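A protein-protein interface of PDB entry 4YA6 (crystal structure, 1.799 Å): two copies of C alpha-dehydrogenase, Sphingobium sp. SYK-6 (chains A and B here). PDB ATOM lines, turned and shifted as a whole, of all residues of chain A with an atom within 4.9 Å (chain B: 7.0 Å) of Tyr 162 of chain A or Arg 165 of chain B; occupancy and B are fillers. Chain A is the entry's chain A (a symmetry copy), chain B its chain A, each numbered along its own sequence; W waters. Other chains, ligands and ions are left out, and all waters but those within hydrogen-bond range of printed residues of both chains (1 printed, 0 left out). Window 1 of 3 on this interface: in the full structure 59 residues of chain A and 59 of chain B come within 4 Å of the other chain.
The side-chain sulfur (SG) of Cys 158 of chain B is in hydrogen-bond range of the backbone carbonyl oxygen (O) of Gly 166 of chain A (3.8 Å). The side-chain sulfur (SG) of Cys 158 of chain A is in hydrogen-bond range of the backbone carbonyl oxygen (O) of Gly 166 of chain B (3.8 Å). OH of Tyr 162 of chain A sits at hydrogen-bond distance from OE2 of Glu 169 of chain B (2.8 Å). The side-chain sulfur (SG) of Cys 158 of chain A sits at hydrogen-bond distance from the side-chain hydroxyl (OG) of Ser 170 of chain B (3.4 Å).
The guanidinium group of Arg 165 of chain B sits at hydrogen-bond distance from the backbone carbonyl oxygen of Ala 147 of chain B, at 2.9 Å. OH of Tyr 162 of chain B is in hydrogen-bond range of O of Phe 148 of chain B. The side-chain carboxylate (OE2) of Glu 169 of chain B is in salt-bridge range of the guanidinium group (NH1) of Arg 165 of chain B (3.1 Å). O of Gly 166 of chain B sits at hydrogen-bond distance from OG of Ser 170 of chain B (2.9 Å). O of Ser 146 of chain A sits at hydrogen-bond distance from SG of Cys 158 of chain A, at 3.4 Å. The guanidinium group (NH2) of Arg 165 of chain A sits at hydrogen-bond distance from the backbone carbonyl oxygen (O) of Ala 147 of chain A (2.9 Å).
Among the printed residues, merely in contact across the chains: Thr 159 of chain A with Ala 163 of chain B, Thr 159 of chain A with Leu 167 of chain B, Tyr 162 of chain A with Tyr 162 of chain B, Tyr 162 of chain A with Arg 165 of chain B, Tyr 162 of chain A with Gly 166 of chain B, Ala 163 of chain A with Thr 159 of chain B, Ala 163 of chain A with Ala 163 of chain B, Arg 165 of chain A with Tyr 162 of chain B and Gly 166 of chain A with Tyr 162 of chain B.
Of chain B, only Tyr 162 (3.4 Å), Arg 165 (3.6 Å), Gly 166 (3.6 Å) and Glu 169 (2.8 Å) come within 4 Å of Tyr 162 of chain A. Arg 165 of chain B touches one residue of chain A. Printed residues of chain B within 4 Å of Thr 159 of chain A: Ala 163 and Leu 167. Of the printed residues of chain A, Tyr 162 of chain B touches Tyr 162 (3.4 Å), Arg 165 (3.6 Å) and Gly 166 (3.6 Å). Ala 143 of chain B touches none of the printed residues of chain A. Phe 247 of chain B touches none of the printed residues of chain A. The nearest residue of chain B that does not touch Tyr 162 of chain A is Ala 163 of chain B (4.5 Å). The nearest printed residue of chain B that does not touch Gly 166 of chain A is Thr 159 of chain B (4.1 Å).
Of the 25 printed residues of chain B, 9 touch a printed residue of chain A. Hydrophobic or aromatic side chains of chain B within 4 Å of the printed part of chain A: Tyr 162, Ala 163 and Leu 167. Hydrophobic or aromatic side chains of chain A within 4 Å of the printed part of chain B: Tyr 162 and Ala 163. Among the printed residues, 13 pairs touch across the chains. Among the printed residues, no Asp or Glu carboxylate lies within 4 Å of a Lys or Arg side-chain nitrogen of the other chain.
Cys 158 of chain A touches Gly 166 of chain B, and with the chains exchanged Gly 166 of chain A touches Cys 158 of chain B. Thr 159 of chain A touches Ala 163 of chain B, and with the chains exchanged Ala 163 of chain A touches Thr 159 of chain B. Tyr 162 of chain A touches its own counterpart, Tyr 162 of chain B. Tyr 162 of chain A touches Gly 166 of chain B, and with the chains exchanged Gly 166 of chain A touches Tyr 162 of chain B. 12 positions are printed for both chains. Of the 13 pairs that touch across the chains among the printed residues, 10 have their exchanged pair printed and touching as well.
Water W1 lies within hydrogen-bond range of OE1 of Glu 169 of chain B (2.8 Å), O of Phe 148 of chain A (2.9 Å) and OH of Tyr 162 of chain A (3.5 Å).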
ATOM      1  N   SER A 146      27.209  36.429  -7.941  1.00  0.00           N
ATOM      2  CA  SER A 146      25.815  36.031  -7.767  1.00  0.00           C
ATOM      3  C   SER A 146      25.674  34.523  -7.548  1.00  0.00           C
ATOM      4  O   SER A 146      24.582  34.037  -7.254  1.00  0.00           O
ATOM      5  CB  SER A 146      24.984  36.457  -8.977  1.00  0.00           C
ATOM      6  OG  SER A 146      24.892  37.870  -9.055  1.00  0.00           O
ATOM      7  N   ALA A 147      26.775  33.790  -7.700  1.00  0.00           N
ATOM      8  CA  ALA A 147      26.803  32.366  -7.377  1.00  0.00           C
ATOM      9  C   ALA A 147      27.050  32.162  -5.880  1.00  0.00           C
ATOM     10  O   ALA A 147      27.164  31.028  -5.410  1.00  0.00           O
ATOM     11  CB  ALA A 147      27.873  31.654  -8.195  1.00  0.00           C
ATOM     12  N   PHE A 148      27.137  33.268  -5.144  1.00  0.00           N
ATOM     13  CA  PHE A 148      27.319  33.239  -3.698  1.00  0.00           C
ATOM     14  C   PHE A 148      26.327  34.149  -2.982  1.00  0.00           C
ATOM     15  O   PHE A 148      25.991  33.915  -1.822  1.00  0.00           O
ATOM     16  CB  PHE A 148      28.742  33.665  -3.327  1.00  0.00           C
ATOM     17  CG  PHE A 148      29.782  32.632  -3.637  1.00  0.00           C
ATOM     18  CD1 PHE A 148      30.125  31.674  -2.700  1.00  0.00           C
ATOM     19  CD2 PHE A 148      30.424  32.623  -4.864  1.00  0.00           C
ATOM     20  CE1 PHE A 148      31.083  30.722  -2.979  1.00  0.00           C
ATOM     21  CE2 PHE A 148      31.384  31.672  -5.149  1.00  0.00           C
ATOM     22  CZ  PHE A 148      31.715  30.722  -4.204  1.00  0.00           C
ATOM     23  N   VAL A 149      25.866  35.185  -3.680  1.00  0.00           N
ATOM     24  CA  VAL A 149      25.077  36.242  -3.054  1.00  0.00           C
ATOM     25  C   VAL A 149      23.805  36.539  -3.835  1.00  0.00           C
ATOM     26  O   VAL A 149      23.856  37.065  -4.946  1.00  0.00           O
ATOM     27  CB  VAL A 149      25.894  37.544  -2.926  1.00  0.00           C
ATOM     28  CG1 VAL A 149      25.156  38.560  -2.064  1.00  0.00           C
ATOM     29  CG2 VAL A 149      27.269  37.251  -2.342  1.00  0.00           C
ATOM     30  N   CYS A 158      20.854  34.876 -10.561  1.00  0.00           N
ATOM     31  CA  CYS A 158      21.413  34.150  -9.427  1.00  0.00           C
ATOM     32  C   CYS A 158      21.231  32.642  -9.587  1.00  0.00           C
ATOM     33  O   CYS A 158      22.163  31.871  -9.359  1.00  0.00           O
ATOM     34  CB  CYS A 158      20.756  34.628  -8.132  1.00  0.00           C
ATOM     35  SG  CYS A 158      21.285  33.756  -6.649  1.00  0.00           S
ATOM     36  N   THR A 159      20.034  32.227  -9.986  1.00  0.00           N
ATOM     37  CA  THR A 159      19.749  30.809 -10.168  1.00  0.00           C
ATOM     38  C   THR A 159      20.686  30.199 -11.215  1.00  0.00           C
ATOM     39  O   THR A 159      21.209  29.103 -11.015  1.00  0.00           O
ATOM     40  CB  THR A 159      18.275  30.577 -10.580  1.00  0.00           C
ATOM     41  OG1 THR A 159      17.407  31.153  -9.597  1.00  0.00           O
ATOM     42  CG2 THR A 159      17.963  29.093 -10.687  1.00  0.00           C
ATOM     43  N   THR A 160      20.924  30.913 -12.315  1.00  0.00           N
ATOM     44  CA  THR A 160      21.765  30.371 -13.385  1.00  0.00           C
ATOM     45  C   THR A 160      23.232  30.293 -12.970  1.00  0.00           C
ATOM     46  O   THR A 160      23.952  29.383 -13.384  1.00  0.00           O
ATOM     47  CB  THR A 160      21.671  31.202 -14.691  1.00  0.00           C
ATOM     48  OG1 THR A 160      22.235  32.505 -14.493  1.00  0.00           O
ATOM     49  CG2 THR A 160      20.227  31.321 -15.159  1.00  0.00           C
ATOM     50  N   LYS A 161      23.680  31.238 -12.150  1.00  0.00           N
ATOM     51  CA  LYS A 161      25.085  31.284 -11.769  1.00  0.00           C
ATOM     52  C   LYS A 161      25.390  30.292 -10.651  1.00  0.00           C
ATOM     53  O   LYS A 161      26.483  29.728 -10.601  1.00  0.00           O
ATOM     54  CB  LYS A 161      25.477  32.707 -11.366  1.00  0.00           C
ATOM     55  CG  LYS A 161      25.416  33.701 -12.528  1.00  0.00           C
ATOM     56  CD  LYS A 161      26.303  33.266 -13.692  1.00  0.00           C
ATOM     57  CE  LYS A 161      26.323  34.289 -14.810  1.00  0.00           C
ATOM     58  NZ  LYS A 161      27.094  33.800 -15.986  1.00  0.00           N
ATOM     59  N   TYR A 162      24.429  30.067  -9.762  1.00  0.00           N
ATOM     60  CA  TYR A 162      24.542  28.974  -8.801  1.00  0.00           C
ATOM     61  C   TYR A 162      24.659  27.649  -9.546  1.00  0.00           C
ATOM     62  O   TYR A 162      25.456  26.785  -9.182  1.00  0.00           O
ATOM     63  CB  TYR A 162      23.336  28.934  -7.863  1.00  0.00           C
ATOM     64  CG  TYR A 162      23.563  29.609  -6.530  1.00  0.00           C
ATOM     65  CD1 TYR A 162      23.553  30.991  -6.422  1.00  0.00           C
ATOM     66  CD2 TYR A 162      23.774  28.863  -5.378  1.00  0.00           C
ATOM     67  CE1 TYR A 162      23.756  31.615  -5.206  1.00  0.00           C
ATOM     68  CE2 TYR A 162      23.978  29.480  -4.156  1.00  0.00           C
ATOM     69  CZ  TYR A 162      23.966  30.854  -4.075  1.00  0.00           C
ATOM     70  OH  TYR A 162      24.165  31.473  -2.863  1.00  0.00           O
ATOM     71  N   ALA A 163      23.854  27.497 -10.593  1.00  0.00           N
ATOM     72  CA  ALA A 163      23.836  26.260 -11.363  1.00  0.00           C
ATOM     73  C   ALA A 163      25.215  25.942 -11.926  1.00  0.00           C
ATOM     74  O   ALA A 163      25.727  24.842 -11.735  1.00  0.00           O
ATOM     75  CB  ALA A 163      22.815  26.350 -12.488  1.00  0.00           C
ATOM     76  N   VAL A 164      25.828  26.901 -12.612  1.00  0.00           N
ATOM     77  CA  VAL A 164      27.116  26.631 -13.244  1.00  0.00           C
ATOM     78  C   VAL A 164      28.221  26.539 -12.197  1.00  0.00           C
ATOM     79  O   VAL A 164      29.260  25.929 -12.442  1.00  0.00           O
ATOM     80  CB  VAL A 164      27.473  27.691 -14.309  1.00  0.00           C
ATOM     81  CG1 VAL A 164      26.486  27.615 -15.469  1.00  0.00           C
ATOM     82  CG2 VAL A 164      27.508  29.084 -13.712  1.00  0.00           C
ATOM     83  N   ARG A 165      27.997  27.122 -11.021  1.00  0.00           N
ATOM     84  CA  ARG A 165      28.924  26.920  -9.915  1.00  0.00           C
ATOM     85  C   ARG A 165      28.922  25.450  -9.502  1.00  0.00           C
ATOM     86  O   ARG A 165      29.976  24.860  -9.270  1.00  0.00           O
ATOM     87  CB  ARG A 165      28.569  27.801  -8.718  1.00  0.00           C
ATOM     88  CG  ARG A 165      29.724  27.942  -7.740  1.00  0.00           C
ATOM     89  CD  ARG A 165      29.451  27.338  -6.384  1.00  0.00           C
ATOM     90  NE  ARG A 165      28.779  28.269  -5.486  1.00  0.00           N
ATOM     91  CZ  ARG A 165      28.850  28.218  -4.159  1.00  0.00           C
ATOM     92  NH1 ARG A 165      29.571  27.283  -3.555  1.00  0.00           N
ATOM     93  NH2 ARG A 165      28.199  29.113  -3.432  1.00  0.00           N
ATOM     94  N   GLY A 166      27.731  24.865  -9.418  1.00  0.00           N
ATOM     95  CA  GLY A 166      27.599  23.452  -9.106  1.00  0.00           C
ATOM     96  C   GLY A 166      28.264  22.584 -10.158  1.00  0.00           C
ATOM     97  O   GLY A 166      28.944  21.611  -9.833  1.00  0.00           O
ATOM     98  N   ILE B 141      11.312  24.665  -0.734  1.00  0.00           N
ATOM     99  CA  ILE B 141      12.066  24.045  -1.812  1.00  0.00           C
ATOM    100  C   ILE B 141      12.922  22.950  -1.199  1.00  0.00           C
ATOM    101  O   ILE B 141      13.721  23.209  -0.300  1.00  0.00           O
ATOM    102  CB  ILE B 141      12.940  25.070  -2.570  1.00  0.00           C
ATOM    103  CG1 ILE B 141      12.048  25.998  -3.397  1.00  0.00           C
ATOM    104  CG2 ILE B 141      13.937  24.368  -3.493  1.00  0.00           C
ATOM    105  CD1 ILE B 141      12.754  27.231  -3.931  1.00  0.00           C
ATOM    106  N   ALA B 143      15.886  20.734  -1.817  1.00  0.00           N
ATOM    107  CA  ALA B 143      17.058  20.534  -2.651  1.00  0.00           C
ATOM    108  C   ALA B 143      17.769  19.245  -2.244  1.00  0.00           C
ATOM    109  O   ALA B 143      17.238  18.153  -2.449  1.00  0.00           O
ATOM    110  CB  ALA B 143      17.990  21.733  -2.554  1.00  0.00           C
ATOM    111  N   SER B 144      18.953  19.378  -1.654  1.00  0.00           N
ATOM    112  CA  SER B 144      19.799  18.239  -1.335  1.00  0.00           C
ATOM    113  C   SER B 144      21.094  18.746  -0.724  1.00  0.00           C
ATOM    114  O   SER B 144      21.466  19.899  -0.927  1.00  0.00           O
ATOM    115  CB  SER B 144      20.097  17.413  -2.590  1.00  0.00           C
ATOM    116  OG  SER B 144      21.058  16.408  -2.330  1.00  0.00           O
ATOM    117  N   ALA B 147      23.538  20.314  -2.933  1.00  0.00           N
ATOM    118  CA  ALA B 147      23.554  21.753  -3.186  1.00  0.00           C
ATOM    119  C   ALA B 147      24.708  22.417  -2.432  1.00  0.00           C
ATOM    120  O   ALA B 147      24.863  23.639  -2.469  1.00  0.00           O
ATOM    121  CB  ALA B 147      22.224  22.380  -2.785  1.00  0.00           C
ATOM    122  N   PHE B 148      25.506  21.601  -1.746  1.00  0.00           N
ATOM    123  CA  PHE B 148      26.677  22.074  -1.018  1.00  0.00           C
ATOM    124  C   PHE B 148      27.917  21.246  -1.336  1.00  0.00           C
ATOM    125  O   PHE B 148      29.040  21.738  -1.231  1.00  0.00           O
ATOM    126  CB  PHE B 148      26.424  22.033   0.491  1.00  0.00           C
ATOM    127  CG  PHE B 148      25.493  23.101   0.978  1.00  0.00           C
ATOM    128  CD1 PHE B 148      25.983  24.333   1.377  1.00  0.00           C
ATOM    129  CD2 PHE B 148      24.130  22.874   1.045  1.00  0.00           C
ATOM    130  CE1 PHE B 148      25.132  25.320   1.828  1.00  0.00           C
ATOM    131  CE2 PHE B 148      23.273  23.858   1.495  1.00  0.00           C
ATOM    132  CZ  PHE B 148      23.775  25.082   1.889  1.00  0.00           C
ATOM    133  N   VAL B 149      27.705  19.989  -1.720  1.00  0.00           N
ATOM    134  CA  VAL B 149      28.799  19.032  -1.854  1.00  0.00           C
ATOM    135  C   VAL B 149      28.755  18.303  -3.189  1.00  0.00           C
ATOM    136  O   VAL B 149      27.857  17.499  -3.439  1.00  0.00           O
ATOM    137  CB  VAL B 149      28.768  17.988  -0.719  1.00  0.00           C
ATOM    138  CG1 VAL B 149      30.038  17.146  -0.728  1.00  0.00           C
ATOM    139  CG2 VAL B 149      28.595  18.676   0.627  1.00  0.00           C
ATOM    140  N   CYS B 158      23.952  17.420  -8.923  1.00  0.00           N
ATOM    141  CA  CYS B 158      24.554  18.527  -8.191  1.00  0.00           C
ATOM    142  C   CYS B 158      24.231  19.869  -8.844  1.00  0.00           C
ATOM    143  O   CYS B 158      23.864  20.826  -8.162  1.00  0.00           O
ATOM    144  CB  CYS B 158      26.069  18.331  -8.108  1.00  0.00           C
ATOM    145  SG  CYS B 158      26.963  19.670  -7.305  1.00  0.00           S
ATOM    146  N   THR B 159      24.357  19.933 -10.164  1.00  0.00           N
ATOM    147  CA  THR B 159      24.076  21.166 -10.892  1.00  0.00           C
ATOM    148  C   THR B 159      22.627  21.607 -10.668  1.00  0.00           C
ATOM    149  O   THR B 159      22.367  22.790 -10.445  1.00  0.00           O
ATOM    150  CB  THR B 159      24.351  21.004 -12.407  1.00  0.00           C
ATOM    151  OG1 THR B 159      25.707  20.588 -12.605  1.00  0.00           O
ATOM    152  CG2 THR B 159      24.137  22.316 -13.145  1.00  0.00           C
ATOM    153  N   THR B 160      21.687  20.663 -10.696  1.00  0.00           N
ATOM    154  CA  THR B 160      20.274  21.018 -10.546  1.00  0.00           C
ATOM    155  C   THR B 160      19.949  21.471  -9.125  1.00  0.00           C
ATOM    156  O   THR B 160      19.097  22.336  -8.924  1.00  0.00           O
ATOM    157  CB  THR B 160      19.327  19.845 -10.912  1.00  0.00           C
ATOM    158  OG1 THR B 160      19.473  18.774  -9.969  1.00  0.00           O
ATOM    159  CG2 THR B 160      19.602  19.341 -12.323  1.00  0.00           C
ATOM    160  N   LYS B 161      20.626  20.895  -8.137  1.00  0.00           N
ATOM    161  CA  LYS B 161      20.323  21.210  -6.748  1.00  0.00           C
ATOM    162  C   LYS B 161      20.981  22.518  -6.319  1.00  0.00           C
ATOM    163  O   LYS B 161      20.422  23.258  -5.508  1.00  0.00           O
ATOM    164  CB  LYS B 161      20.747  20.056  -5.838  1.00  0.00           C
ATOM    165  CG  LYS B 161      19.940  18.776  -6.071  1.00  0.00           C
ATOM    166  CD  LYS B 161      18.443  19.011  -5.889  1.00  0.00           C
ATOM    167  CE  LYS B 161      17.642  17.731  -6.026  1.00  0.00           C
ATOM    168  NZ  LYS B 161      16.177  17.993  -5.964  1.00  0.00           N
ATOM    169  N   TYR B 162      22.155  22.813  -6.866  1.00  0.00           N
ATOM    170  CA  TYR B 162      22.745  24.138  -6.695  1.00  0.00           C
ATOM    171  C   TYR B 162      21.808  25.192  -7.270  1.00  0.00           C
ATOM    172  O   TYR B 162      21.606  26.252  -6.677  1.00  0.00           O
ATOM    173  CB  TYR B 162      24.108  24.229  -7.383  1.00  0.00           C
ATOM    174  CG  TYR B 162      25.285  24.014  -6.459  1.00  0.00           C
ATOM    175  CD1 TYR B 162      25.630  22.742  -6.029  1.00  0.00           C
ATOM    176  CD2 TYR B 162      26.059  25.084  -6.029  1.00  0.00           C
ATOM    177  CE1 TYR B 162      26.707  22.538  -5.188  1.00  0.00           C
ATOM    178  CE2 TYR B 162      27.140  24.889  -5.185  1.00  0.00           C
ATOM    179  CZ  TYR B 162      27.459  23.615  -4.771  1.00  0.00           C
ATOM    180  OH  TYR B 162      28.534  23.415  -3.936  1.00  0.00           O
ATOM    181  N   ALA B 163      21.238  24.894  -8.432  1.00  0.00           N
ATOM    182  CA  ALA B 163      20.354  25.834  -9.110  1.00  0.00           C
ATOM    183  C   ALA B 163      19.176  26.218  -8.224  1.00  0.00           C
ATOM    184  O   ALA B 163      18.912  27.400  -8.018  1.00  0.00           O
ATOM    185  CB  ALA B 163      19.858  25.246 -10.424  1.00  0.00           C
ATOM    186  N   VAL B 164      18.469  25.228  -7.690  1.00  0.00           N
ATOM    187  CA  VAL B 164      17.280  25.531  -6.899  1.00  0.00           C
ATOM    188  C   VAL B 164      17.670  26.114  -5.544  1.00  0.00           C
ATOM    189  O   VAL B 164      16.871  26.803  -4.911  1.00  0.00           O
ATOM    190  CB  VAL B 164      16.378  24.291  -6.710  1.00  0.00           C
ATOM    191  CG1 VAL B 164      15.806  23.856  -8.054  1.00  0.00           C
ATOM    192  CG2 VAL B 164      17.129  23.157  -6.043  1.00  0.00           C
ATOM    193  N   ARG B 165      18.900  25.862  -5.103  1.00  0.00           N
ATOM    194  CA  ARG B 165      19.403  26.532  -3.911  1.00  0.00           C
ATOM    195  C   ARG B 165      19.502  28.033  -4.168  1.00  0.00           C
ATOM    196  O   ARG B 165      19.117  28.843  -3.326  1.00  0.00           O
ATOM    197  CB  ARG B 165      20.765  25.982  -3.490  1.00  0.00           C
ATOM    198  CG  ARG B 165      21.113  26.334  -2.053  1.00  0.00           C
ATOM    199  CD  ARG B 165      22.311  27.242  -1.921  1.00  0.00           C
ATOM    200  NE  ARG B 165      23.567  26.502  -1.882  1.00  0.00           N
ATOM    201  CZ  ARG B 165      24.681  26.942  -1.304  1.00  0.00           C
ATOM    202  NH1 ARG B 165      24.711  28.124  -0.702  1.00  0.00           N
ATOM    203  NH2 ARG B 165      25.772  26.192  -1.324  1.00  0.00           N
ATOM    204  N   GLY B 166      20.017  28.397  -5.338  1.00  0.00           N
ATOM    205  CA  GLY B 166      20.097  29.793  -5.733  1.00  0.00           C
ATOM    206  C   GLY B 166      18.722  30.428  -5.822  1.00  0.00           C
ATOM    207  O   GLY B 166      18.520  31.558  -5.378  1.00  0.00           O
ATOM    208  N   LEU B 167      17.770  29.700  -6.399  1.00  0.00           N
ATOM    209  CA  LEU B 167      16.396  30.177  -6.492  1.00  0.00           C
ATOM    210  C   LEU B 167      15.822  30.408  -5.097  1.00  0.00           C
ATOM    211  O   LEU B 167      15.169  31.421  -4.845  1.00  0.00           O
ATOM    212  CB  LEU B 167      15.527  29.180  -7.263  1.00  0.00           C
ATOM    213  CG  LEU B 167      14.030  29.494  -7.346  1.00  0.00           C
ATOM    214  CD1 LEU B 167      13.781  30.872  -7.938  1.00  0.00           C
ATOM    215  CD2 LEU B 167      13.316  28.431  -8.162  1.00  0.00           C
ATOM    216  N   ALA B 168      16.076  29.463  -4.194  1.00  0.00           N
ATOM    217  CA  ALA B 168      15.591  29.561  -2.823  1.00  0.00           C
ATOM    218  C   ALA B 168      16.162  30.788  -2.117  1.00  0.00           C
ATOM    219  O   ALA B 168      15.431  31.524  -1.453  1.00  0.00           O
ATOM    220  CB  ALA B 168      15.937  28.300  -2.045  1.00  0.00           C
ATOM    221  N   GLU B 169      17.467  31.005  -2.254  1.00  0.00           N
ATOM    222  CA  GLU B 169      18.104  32.150  -1.611  1.00  0.00           C
ATOM    223  C   GLU B 169      17.628  33.457  -2.243  1.00  0.00           C
ATOM    224  O   GLU B 169      17.632  34.500  -1.595  1.00  0.00           O
ATOM    225  CB  GLU B 169      19.628  32.048  -1.692  1.00  0.00           C
ATOM    226  CG  GLU B 169      20.205  30.884  -0.899  1.00  0.00           C
ATOM    227  CD  GLU B 169      21.690  31.024  -0.640  1.00  0.00           C
ATOM    228  OE1 GLU B 169      22.090  31.996   0.036  1.00  0.00           O
ATOM    229  OE2 GLU B 169      22.458  30.158  -1.108  1.00  0.00           O
ATOM    230  N   SER B 170      17.212  33.392  -3.504  1.00  0.00           N
ATOM    231  CA  SER B 170      16.677  34.564  -4.193  1.00  0.00           C
ATOM    232  C   SER B 170      15.278  34.893  -3.687  1.00  0.00           C
ATOM    233  O   SER B 170      14.955  36.051  -3.435  1.00  0.00           O
ATOM    234  CB  SER B 170      16.650  34.334  -5.704  1.00  0.00           C
ATOM    235  OG  SER B 170      17.963  34.238  -6.223  1.00  0.00           O
ATOM    236  N   LEU B 171      14.449  33.866  -3.546  1.00  0.00           N
ATOM    237  CA  LEU B 171      13.118  34.023  -2.971  1.00  0.00           C
ATOM    238  C   LEU B 171      13.213  34.590  -1.557  1.00  0.00           C
ATOM    239  O   LEU B 171      12.400  35.425  -1.153  1.00  0.00           O
ATOM    240  CB  LEU B 171      12.385  32.675  -2.949  1.00  0.00           C
ATOM    241  CG  LEU B 171      11.213  32.375  -3.899  1.00  0.00           C
ATOM    242  CD1 LEU B 171      11.095  33.325  -5.079  1.00  0.00           C
ATOM    243  CD2 LEU B 171      11.328  30.938  -4.400  1.00  0.00           C
ATOM    244  N   LEU B 184      14.398  26.180   2.765  1.00  0.00           N
ATOM    245  CA  LEU B 184      15.209  25.332   1.902  1.00  0.00           C
ATOM    246  C   LEU B 184      15.652  24.083   2.655  1.00  0.00           C
ATOM    247  O   LEU B 184      16.473  24.155   3.570  1.00  0.00           O
ATOM    248  CB  LEU B 184      16.426  26.096   1.385  1.00  0.00           C
ATOM    249  CG  LEU B 184      17.382  25.282   0.510  1.00  0.00           C
ATOM    250  CD1 LEU B 184      16.702  24.803  -0.764  1.00  0.00           C
ATOM    251  CD2 LEU B 184      18.598  26.104   0.179  1.00  0.00           C
ATOM    252  N   CYS B 186      17.495  20.430   2.756  1.00  0.00           N
ATOM    253  CA  CYS B 186      18.545  19.638   2.123  1.00  0.00           C
ATOM    254  C   CYS B 186      18.660  18.273   2.799  1.00  0.00           C
ATOM    255  O   CYS B 186      19.429  18.114   3.746  1.00  0.00           O
ATOM    256  CB  CYS B 186      19.884  20.374   2.183  1.00  0.00           C
ATOM    257  SG  CYS B 186      19.888  21.971   1.341  1.00  0.00           S
ATOM    258  N   PHE B 247      14.700  29.367   7.263  1.00  0.00           N
ATOM    259  CA  PHE B 247      15.134  29.186   5.887  1.00  0.00           C
ATOM    260  C   PHE B 247      16.033  27.964   5.735  1.00  0.00           C
ATOM    261  O   PHE B 247      15.720  27.052   4.970  1.00  0.00           O
ATOM    262  CB  PHE B 247      15.869  30.425   5.376  1.00  0.00           C
ATOM    263  CG  PHE B 247      16.379  30.276   3.973  1.00  0.00           C
ATOM    264  CD1 PHE B 247      15.515  30.374   2.896  1.00  0.00           C
ATOM    265  CD2 PHE B 247      17.718  30.019   3.731  1.00  0.00           C
ATOM    266  CE1 PHE B 247      15.976  30.225   1.603  1.00  0.00           C
ATOM    267  CE2 PHE B 247      18.186  29.871   2.441  1.00  0.00           C
ATOM    268  CZ  PHE B 247      17.314  29.975   1.374  1.00  0.00           C
ATOM    269  N   TRP B 248      17.156  27.954   6.445  1.00  0.00           N
ATOM    270  CA  TRP B 248      18.102  26.847   6.345  1.00  0.00           C
ATOM    271  C   TRP B 248      17.613  25.640   7.134  1.00  0.00           C
ATOM    272  O   TRP B 248      17.610  25.656   8.365  1.00  0.00           O
ATOM    273  CB  TRP B 248      19.487  27.259   6.847  1.00  0.00           C
ATOM    274  CG  TRP B 248      20.173  28.291   6.000  1.00  0.00           C
ATOM    275  CD1 TRP B 248      20.516  29.559   6.372  1.00  0.00           C
ATOM    276  CD2 TRP B 248      20.603  28.142   4.642  1.00  0.00           C
ATOM    277  NE1 TRP B 248      21.134  30.207   5.330  1.00  0.00           N
ATOM    278  CE2 TRP B 248      21.199  29.360   4.255  1.00  0.00           C
ATOM    279  CE3 TRP B 248      20.543  27.099   3.713  1.00  0.00           C
ATOM    280  CZ2 TRP B 248      21.729  29.560   2.983  1.00  0.00           C
ATOM    281  CZ3 TRP B 248      21.071  27.301   2.453  1.00  0.00           C
ATOM    282  CH2 TRP B 248      21.655  28.523   2.099  1.00  0.00           C
ATOM    283  N   GLN B 259      31.786  21.267   6.138  1.00  0.00           N
ATOM    284  CA  GLN B 259      31.332  22.457   5.428  1.00  0.00           C
ATOM    285  C   GLN B 259      32.221  23.653   5.757  1.00  0.00           C
ATOM    286  O   GLN B 259      32.493  24.482   4.889  1.00  0.00           O
ATOM    287  CB  GLN B 259      29.872  22.762   5.772  1.00  0.00           C
ATOM    288  CG  GLN B 259      29.249  23.864   4.925  1.00  0.00           C
ATOM    289  CD  GLN B 259      29.269  23.546   3.441  1.00  0.00           C
ATOM    290  OE1 GLN B 259      28.983  22.421   3.030  1.00  0.00           O
ATOM    291  NE2 GLN B 259      29.616  24.537   2.632  1.00  0.00           N
HETATM  292  O   HOH W   1      23.262  34.308  -1.029  1.00  0.00           O
